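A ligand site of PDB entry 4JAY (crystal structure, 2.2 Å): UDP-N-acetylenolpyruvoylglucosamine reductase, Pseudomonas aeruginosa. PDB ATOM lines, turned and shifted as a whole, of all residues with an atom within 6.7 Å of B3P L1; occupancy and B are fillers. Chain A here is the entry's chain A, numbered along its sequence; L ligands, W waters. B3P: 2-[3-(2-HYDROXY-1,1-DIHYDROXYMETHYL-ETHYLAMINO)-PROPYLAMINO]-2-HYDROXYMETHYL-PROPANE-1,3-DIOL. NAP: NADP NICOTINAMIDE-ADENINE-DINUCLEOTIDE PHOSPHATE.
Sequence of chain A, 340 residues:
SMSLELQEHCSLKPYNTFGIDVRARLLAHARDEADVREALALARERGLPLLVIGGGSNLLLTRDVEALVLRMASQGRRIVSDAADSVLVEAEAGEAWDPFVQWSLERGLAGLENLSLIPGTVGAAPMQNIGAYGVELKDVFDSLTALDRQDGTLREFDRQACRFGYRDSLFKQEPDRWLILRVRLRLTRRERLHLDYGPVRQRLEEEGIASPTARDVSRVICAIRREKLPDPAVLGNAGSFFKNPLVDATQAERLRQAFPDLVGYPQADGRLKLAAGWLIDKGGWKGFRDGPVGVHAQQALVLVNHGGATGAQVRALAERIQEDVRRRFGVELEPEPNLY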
ATOM      1  N   GLY A 131      20.497  15.785 -29.279  1.00  0.00           N
ATOM      2  CA  GLY A 131      20.628  15.354 -27.896  1.00  0.00           C
ATOM      3  C   GLY A 131      19.379  15.602 -27.098  1.00  0.00           C
ATOM      4  O   GLY A 131      18.649  16.560 -27.361  1.00  0.00           O
ATOM      5  N   ALA A 132      19.192  14.780 -26.095  1.00  0.00           N
ATOM      6  CA  ALA A 132      18.122  14.934 -25.128  1.00  0.00           C
ATOM      7  C   ALA A 132      18.431  14.016 -23.927  1.00  0.00           C
ATOM      8  O   ALA A 132      18.993  12.961 -24.085  1.00  0.00           O
ATOM      9  CB  ALA A 132      16.789  14.534 -25.743  1.00  0.00           C
ATOM     10  N   TYR A 133      18.034  14.426 -22.741  1.00  0.00           N
ATOM     11  CA  TYR A 133      18.167  13.625 -21.577  1.00  0.00           C
ATOM     12  C   TYR A 133      19.597  13.149 -21.338  1.00  0.00           C
ATOM     13  O   TYR A 133      19.813  12.020 -20.923  1.00  0.00           O
ATOM     14  CB  TYR A 133      17.087  12.510 -21.619  1.00  0.00           C
ATOM     15  CG  TYR A 133      15.714  13.147 -21.574  1.00  0.00           C
ATOM     16  CD1 TYR A 133      15.258  13.824 -20.439  1.00  0.00           C
ATOM     17  CD2 TYR A 133      14.893  13.158 -22.681  1.00  0.00           C
ATOM     18  CE1 TYR A 133      14.025  14.446 -20.419  1.00  0.00           C
ATOM     19  CE2 TYR A 133      13.646  13.783 -22.649  1.00  0.00           C
ATOM     20  CZ  TYR A 133      13.219  14.418 -21.509  1.00  0.00           C
ATOM     21  OH  TYR A 133      11.984  15.077 -21.506  1.00  0.00           O
ATOM     22  N   GLY A 134      20.571  14.034 -21.559  1.00  0.00           N
ATOM     23  CA  GLY A 134      21.978  13.763 -21.256  1.00  0.00           C
ATOM     24  C   GLY A 134      22.715  12.906 -22.257  1.00  0.00           C
ATOM     25  O   GLY A 134      23.834  12.467 -22.015  1.00  0.00           O
ATOM     26  N   VAL A 135      22.085  12.589 -23.378  1.00  0.00           N
ATOM     27  CA  VAL A 135      22.734  11.810 -24.416  1.00  0.00           C
ATOM     28  C   VAL A 135      22.781  12.655 -25.676  1.00  0.00           C
ATOM     29  O   VAL A 135      21.866  13.400 -25.972  1.00  0.00           O
ATOM     30  CB  VAL A 135      22.004  10.469 -24.685  1.00  0.00           C
ATOM     31  CG1 VAL A 135      22.610   9.776 -25.875  1.00  0.00           C
ATOM     32  CG2 VAL A 135      22.123   9.547 -23.476  1.00  0.00           C
ATOM     33  N   GLU A 136      23.859  12.492 -26.413  1.00  0.00           N
ATOM     34  CA  GLU A 136      24.029  13.131 -27.695  1.00  0.00           C
ATOM     35  C   GLU A 136      24.428  12.094 -28.721  1.00  0.00           C
ATOM     36  O   GLU A 136      25.095  11.126 -28.413  1.00  0.00           O
ATOM     37  CB  GLU A 136      25.137  14.152 -27.610  1.00  0.00           C
ATOM     38  CG  GLU A 136      24.679  15.469 -27.056  1.00  0.00           C
ATOM     39  CD  GLU A 136      25.791  16.498 -27.022  1.00  0.00           C
ATOM     40  OE1 GLU A 136      26.990  16.098 -26.987  1.00  0.00           O
ATOM     41  OE2 GLU A 136      25.456  17.704 -27.008  1.00  0.00           O
ATOM     42  N   LYS A 138      26.798  12.091 -30.652  1.00  0.00           N
ATOM     43  CA  LYS A 138      28.224  11.812 -30.694  1.00  0.00           C
ATOM     44  C   LYS A 138      28.618  10.660 -29.795  1.00  0.00           C
ATOM     45  O   LYS A 138      29.605  10.025 -30.063  1.00  0.00           O
ATOM     46  CB  LYS A 138      29.081  13.007 -30.314  1.00  0.00           C
ATOM     47  CG  LYS A 138      28.955  13.396 -28.864  1.00  0.00           C
ATOM     48  CD  LYS A 138      29.993  14.408 -28.471  1.00  0.00           C
ATOM     49  CE  LYS A 138      30.025  14.543 -26.948  1.00  0.00           C
ATOM     50  NZ  LYS A 138      30.293  15.959 -26.601  1.00  0.00           N
ATOM     51  N   ASP A 139      27.844  10.410 -28.746  1.00  0.00           N
ATOM     52  CA  ASP A 139      28.191   9.374 -27.766  1.00  0.00           C
ATOM     53  C   ASP A 139      28.101   7.972 -28.381  1.00  0.00           C
ATOM     54  O   ASP A 139      28.731   7.059 -27.915  1.00  0.00           O
ATOM     55  CB  ASP A 139      27.276   9.429 -26.517  1.00  0.00           C
ATOM     56  CG  ASP A 139      27.298  10.798 -25.796  1.00  0.00           C
ATOM     57  OD1 ASP A 139      28.352  11.477 -25.754  1.00  0.00           O
ATOM     58  OD2 ASP A 139      26.239  11.172 -25.232  1.00  0.00           O
ATOM     59  N   TYR A 166      28.173  20.940 -28.477  1.00  0.00           N
ATOM     60  CA  TYR A 166      26.807  21.135 -27.982  1.00  0.00           C
ATOM     61  C   TYR A 166      25.988  21.855 -29.094  1.00  0.00           C
ATOM     62  O   TYR A 166      26.295  22.994 -29.458  1.00  0.00           O
ATOM     63  CB  TYR A 166      26.828  21.892 -26.628  1.00  0.00           C
ATOM     64  CG  TYR A 166      25.467  22.254 -26.206  1.00  0.00           C
ATOM     65  CD1 TYR A 166      24.548  21.266 -25.815  1.00  0.00           C
ATOM     66  CD2 TYR A 166      25.054  23.552 -26.281  1.00  0.00           C
ATOM     67  CE1 TYR A 166      23.252  21.595 -25.471  1.00  0.00           C
ATOM     68  CE2 TYR A 166      23.753  23.904 -25.956  1.00  0.00           C
ATOM     69  CZ  TYR A 166      22.852  22.926 -25.556  1.00  0.00           C
ATOM     70  OH  TYR A 166      21.559  23.321 -25.239  1.00  0.00           O
ATOM     71  N   ARG A 192      22.825  -0.812 -20.838  1.00  0.00           N
ATOM     72  CA  ARG A 192      23.367   0.526 -20.562  1.00  0.00           C
ATOM     73  C   ARG A 192      22.224   1.408 -20.205  1.00  0.00           C
ATOM     74  O   ARG A 192      21.235   1.458 -20.911  1.00  0.00           O
ATOM     75  CB  ARG A 192      24.047   1.178 -21.782  1.00  0.00           C
ATOM     76  CG  ARG A 192      25.135   0.383 -22.481  1.00  0.00           C
ATOM     77  CD  ARG A 192      26.381   0.282 -21.642  1.00  0.00           C
ATOM     78  NE  ARG A 192      26.976   1.572 -21.383  1.00  0.00           N
ATOM     79  CZ  ARG A 192      27.895   2.160 -22.146  1.00  0.00           C
ATOM     80  NH1 ARG A 192      28.327   1.574 -23.274  1.00  0.00           N
ATOM     81  NH2 ARG A 192      28.372   3.349 -21.771  1.00  0.00           N
ATOM     82  N   LEU A 193      22.389   2.173 -19.136  1.00  0.00           N
ATOM     83  CA  LEU A 193      21.394   3.145 -18.729  1.00  0.00           C
ATOM     84  C   LEU A 193      22.065   4.469 -18.435  1.00  0.00           C
ATOM     85  O   LEU A 193      23.027   4.518 -17.691  1.00  0.00           O
ATOM     86  CB  LEU A 193      20.681   2.673 -17.486  1.00  0.00           C
ATOM     87  CG  LEU A 193      19.905   1.365 -17.577  1.00  0.00           C
ATOM     88  CD1 LEU A 193      19.448   0.957 -16.175  1.00  0.00           C
ATOM     89  CD2 LEU A 193      18.708   1.473 -18.512  1.00  0.00           C
ATOM     90  N   HIS A 194      21.575   5.538 -19.048  1.00  0.00           N
ATOM     91  CA  HIS A 194      22.038   6.870 -18.744  1.00  0.00           C
ATOM     92  C   HIS A 194      20.864   7.591 -18.100  1.00  0.00           C
ATOM     93  O   HIS A 194      20.051   8.197 -18.795  1.00  0.00           O
ATOM     94  CB  HIS A 194      22.525   7.593 -20.012  1.00  0.00           C
ATOM     95  CG  HIS A 194      23.538   6.831 -20.793  1.00  0.00           C
ATOM     96  ND1 HIS A 194      24.876   6.797 -20.442  1.00  0.00           N
ATOM     97  CD2 HIS A 194      23.421   6.028 -21.878  1.00  0.00           C
ATOM     98  CE1 HIS A 194      25.542   6.046 -21.299  1.00  0.00           C
ATOM     99  NE2 HIS A 194      24.679   5.561 -22.175  1.00  0.00           N
ATOM    100  N   LEU A 195      20.743   7.520 -16.784  1.00  0.00           N
ATOM    101  CA  LEU A 195      19.552   8.033 -16.099  1.00  0.00           C
ATOM    102  C   LEU A 195      19.893   9.351 -15.412  1.00  0.00           C
ATOM    103  O   LEU A 195      19.421   9.628 -14.326  1.00  0.00           O
ATOM    104  CB  LEU A 195      19.044   7.026 -15.085  1.00  0.00           C
ATOM    105  CG  LEU A 195      18.597   5.683 -15.622  1.00  0.00           C
ATOM    106  CD1 LEU A 195      18.103   4.756 -14.505  1.00  0.00           C
ATOM    107  CD2 LEU A 195      17.501   5.866 -16.643  1.00  0.00           C
ATOM    108  N   ASP A 196      20.662  10.192 -16.108  1.00  0.00           N
ATOM    109  CA  ASP A 196      21.155  11.445 -15.570  1.00  0.00           C
ATOM    110  C   ASP A 196      20.079  12.413 -15.165  1.00  0.00           C
ATOM    111  O   ASP A 196      20.250  13.122 -14.210  1.00  0.00           O
ATOM    112  CB  ASP A 196      22.024  12.174 -16.603  1.00  0.00           C
ATOM    113  CG  ASP A 196      23.135  11.326 -17.126  1.00  0.00           C
ATOM    114  OD1 ASP A 196      24.265  11.856 -17.229  1.00  0.00           O
ATOM    115  OD2 ASP A 196      22.876  10.139 -17.433  1.00  0.00           O
ATOM    116  N   TYR A 197      19.024  12.559 -15.940  1.00  0.00           N
ATOM    117  CA  TYR A 197      18.047  13.633 -15.690  1.00  0.00           C
ATOM    118  C   TYR A 197      17.043  13.086 -14.715  1.00  0.00           C
ATOM    119  O   TYR A 197      16.458  12.054 -14.982  1.00  0.00           O
ATOM    120  CB  TYR A 197      17.335  14.098 -16.996  1.00  0.00           C
ATOM    121  CG  TYR A 197      18.164  15.011 -17.875  1.00  0.00           C
ATOM    122  CD1 TYR A 197      19.529  14.820 -17.987  1.00  0.00           C
ATOM    123  CD2 TYR A 197      17.580  16.032 -18.602  1.00  0.00           C
ATOM    124  CE1 TYR A 197      20.308  15.619 -18.777  1.00  0.00           C
ATOM    125  CE2 TYR A 197      18.350  16.841 -19.420  1.00  0.00           C
ATOM    126  CZ  TYR A 197      19.720  16.625 -19.504  1.00  0.00           C
ATOM    127  OH  TYR A 197      20.568  17.394 -20.272  1.00  0.00           O
ATOM    128  N   GLN A 267      29.998  23.011 -16.156  1.00  0.00           N
ATOM    129  CA  GLN A 267      30.485  22.017 -17.058  1.00  0.00           C
ATOM    130  C   GLN A 267      31.780  21.487 -16.487  1.00  0.00           C
ATOM    131  O   GLN A 267      32.413  22.137 -15.640  1.00  0.00           O
ATOM    132  CB  GLN A 267      30.707  22.676 -18.425  1.00  0.00           C
ATOM    133  CG  GLN A 267      29.431  23.190 -19.069  1.00  0.00           C
ATOM    134  CD  GLN A 267      28.483  22.078 -19.446  1.00  0.00           C
ATOM    135  OE1 GLN A 267      28.683  21.386 -20.426  1.00  0.00           O
ATOM    136  NE2 GLN A 267      27.435  21.908 -18.659  1.00  0.00           N
HETATM  137  C1  B3P L   1      26.212  12.568 -19.757  1.00  0.00           C
HETATM  138  C2  B3P L   1      26.928  13.710 -20.442  1.00  0.00           C
HETATM  139  C3  B3P L   1      27.114  11.380 -19.532  1.00  0.00           C
HETATM  140  N1  B3P L   1      26.438  10.511 -18.595  1.00  0.00           N
HETATM  141  C4  B3P L   1      27.163   9.706 -17.589  1.00  0.00           C
HETATM  142  C5  B3P L   1      28.186   8.876 -18.354  1.00  0.00           C
HETATM  143  C6  B3P L   1      27.798  10.580 -16.490  1.00  0.00           C
HETATM  144  C7  B3P L   1      26.166   8.775 -16.886  1.00  0.00           C
HETATM  145  N2  B3P L   1      26.199  14.195 -21.605  1.00  0.00           N
HETATM  146  C8  B3P L   1      26.840  15.058 -22.589  1.00  0.00           C
HETATM  147  C9  B3P L   1      27.908  14.299 -23.405  1.00  0.00           C
HETATM  148  C10 B3P L   1      27.508  16.210 -21.851  1.00  0.00           C
HETATM  149  C11 B3P L   1      25.749  15.607 -23.531  1.00  0.00           C
HETATM  150  O1  B3P L   1      27.386  13.043 -23.870  1.00  0.00           O
HETATM  151  O2  B3P L   1      28.037  17.076 -22.865  1.00  0.00           O
HETATM  152  O3  B3P L   1      24.447  15.381 -22.974  1.00  0.00           O
HETATM  153  O4  B3P L   1      27.627   8.526 -19.626  1.00  0.00           O
HETATM  154  O5  B3P L   1      29.164  10.950 -16.795  1.00  0.00           O
HETATM  155  O6  B3P L   1      25.006   8.583 -17.708  1.00  0.00           O
HETATM  156  PA  NAP L   2      14.157  19.853 -18.871  1.00  0.00           P
HETATM  157  O1A NAP L   2      14.250  18.353 -18.945  1.00  0.00           O
HETATM  158  O2A NAP L   2      12.934  20.431 -18.199  1.00  0.00           O
HETATM  159  O5B NAP L   2      15.531  20.539 -18.436  1.00  0.00           O
HETATM  160  C5B NAP L   2      15.526  21.960 -18.535  1.00  0.00           C
HETATM  161  C4B NAP L   2      16.898  22.519 -18.881  1.00  0.00           C
HETATM  162  O4B NAP L   2      17.860  22.134 -17.908  1.00  0.00           O
HETATM  163  C3B NAP L   2      17.473  22.046 -20.178  1.00  0.00           C
HETATM  164  O3B NAP L   2      18.161  23.189 -20.731  1.00  0.00           O
HETATM  165  C2B NAP L   2      18.487  20.969 -19.879  1.00  0.00           C
HETATM  166  O2B NAP L   2      19.568  21.072 -20.824  1.00  0.00           O
HETATM  167  C1B NAP L   2      18.871  21.307 -18.450  1.00  0.00           C
HETATM  168  N9A NAP L   2      18.971  20.151 -17.502  1.00  0.00           N
HETATM  169  C8A NAP L   2      17.968  19.540 -16.802  1.00  0.00           C
HETATM  170  N7A NAP L   2      18.454  18.525 -16.056  1.00  0.00           N
HETATM  171  C5A NAP L   2      19.779  18.512 -16.276  1.00  0.00           C
HETATM  172  C6A NAP L   2      20.907  17.695 -15.813  1.00  0.00           C
HETATM  173  N6A NAP L   2      20.659  16.680 -14.945  1.00  0.00           N
HETATM  174  N1A NAP L   2      22.143  17.990 -16.310  1.00  0.00           N
HETATM  175  C2A NAP L   2      22.379  19.007 -17.167  1.00  0.00           C
HETATM  176  N3A NAP L   2      21.383  19.788 -17.604  1.00  0.00           N
HETATM  177  C4A NAP L   2      20.115  19.568 -17.221  1.00  0.00           C
HETATM  178  O3  NAP L   2      14.154  20.440 -20.370  1.00  0.00           O
HETATM  179  PN  NAP L   2      12.989  20.068 -21.432  1.00  0.00           P
HETATM  180  O1N NAP L   2      12.925  21.349 -22.216  1.00  0.00           O
HETATM  181  O2N NAP L   2      11.870  19.370 -20.624  1.00  0.00           O
HETATM  182  O5D NAP L   2      13.733  19.022 -22.412  1.00  0.00           O
HETATM  183  C5D NAP L   2      14.007  17.673 -22.045  1.00  0.00           C
HETATM  184  C4D NAP L   2      15.269  17.247 -22.782  1.00  0.00           C
HETATM  185  O4D NAP L   2      14.883  17.246 -24.143  1.00  0.00           O
HETATM  186  C3D NAP L   2      16.448  18.211 -22.737  1.00  0.00           C
HETATM  187  O3D NAP L   2      17.662  17.450 -22.813  1.00  0.00           O
HETATM  188  C2D NAP L   2      16.260  19.090 -23.962  1.00  0.00           C
HETATM  189  O2D NAP L   2      17.469  19.504 -24.602  1.00  0.00           O
HETATM  190  C1D NAP L   2      15.567  18.173 -24.917  1.00  0.00           C
HETATM  191  N1N NAP L   2      14.621  18.813 -25.829  1.00  0.00           N
HETATM  192  C2N NAP L   2      15.181  19.449 -26.857  1.00  0.00           C
HETATM  193  C3N NAP L   2      14.403  20.083 -27.816  1.00  0.00           C
HETATM  194  C7N NAP L   2      15.056  20.746 -28.973  1.00  0.00           C
HETATM  195  O7N NAP L   2      14.333  21.178 -29.846  1.00  0.00           O
HETATM  196  N7N NAP L   2      16.347  20.836 -29.033  1.00  0.00           N
HETATM  197  C4N NAP L   2      13.008  20.008 -27.745  1.00  0.00           C
HETATM  198  C5N NAP L   2      12.446  19.328 -26.658  1.00  0.00           C
HETATM  199  C6N NAP L   2      13.285  18.745 -25.693  1.00  0.00           C
HETATM  200  P2B NAP L   2      19.734  20.313 -22.266  1.00  0.00           P
HETATM  201  O1X NAP L   2      18.579  20.823 -23.124  1.00  0.00           O
HETATM  202  O2X NAP L   2      21.174  20.818 -22.481  1.00  0.00           O
HETATM  203  O3X NAP L   2      19.601  18.854 -22.096  1.00  0.00           O
HETATM  204  O   HOH W   1      24.798  10.031 -20.884  1.00  0.00           O
HETATM  205  O   HOH W   2      26.890  18.603 -24.939  1.00  0.00           O
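The backbone NH of Tyr 133 sits at hydrogen-bond distance from an oxygen (O3D) of NAP L2 (3.0 Å). An oxygen (O6) of B3P L1 is in hydrogen-bond range of a ring nitrogen (ND1) of His 194, at 3.3 Å. The side-chain carboxylate (OD2) of Asp 139 sits at hydrogen-bond distance from an oxygen (O1) of B3P L1 (2.6 Å). The side-chain hydroxyl of Tyr 197 sits at hydrogen-bond distance from an oxygen (O3X) of NAP L2. The side-chain carboxylate of Asp 196 lies within salt-bridge range of a nitrogen (N1) of B3P L1, 2.9 Å away. A nitrogen (N2) of B3P L1 lies within hydrogen-bond range of the backbone carbonyl oxygen (O) of Gly 134 (3.0 Å).
OE1 of Glu 136 is in salt-bridge range of NZ of Lys 138, 3.3 Å away. N of Glu 136 lies within hydrogen-bond range of OD2 of Asp 139, at 3.0 Å.
N of Val 135 touches O3 of B3P L1 (3.7 Å). CD of Glu 136 touches C11 of B3P L1, at 3.6 Å.
Water W2 lies within hydrogen-bond range of the side-chain carboxylate of Glu 136 and an oxygen (O2) of B3P L1. Water W1 lies within hydrogen-bond range of O of Gly 134 (2.9 Å), N1 of B3P L1 (2.9 Å) and ND1 of His 194 (3.3 Å).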
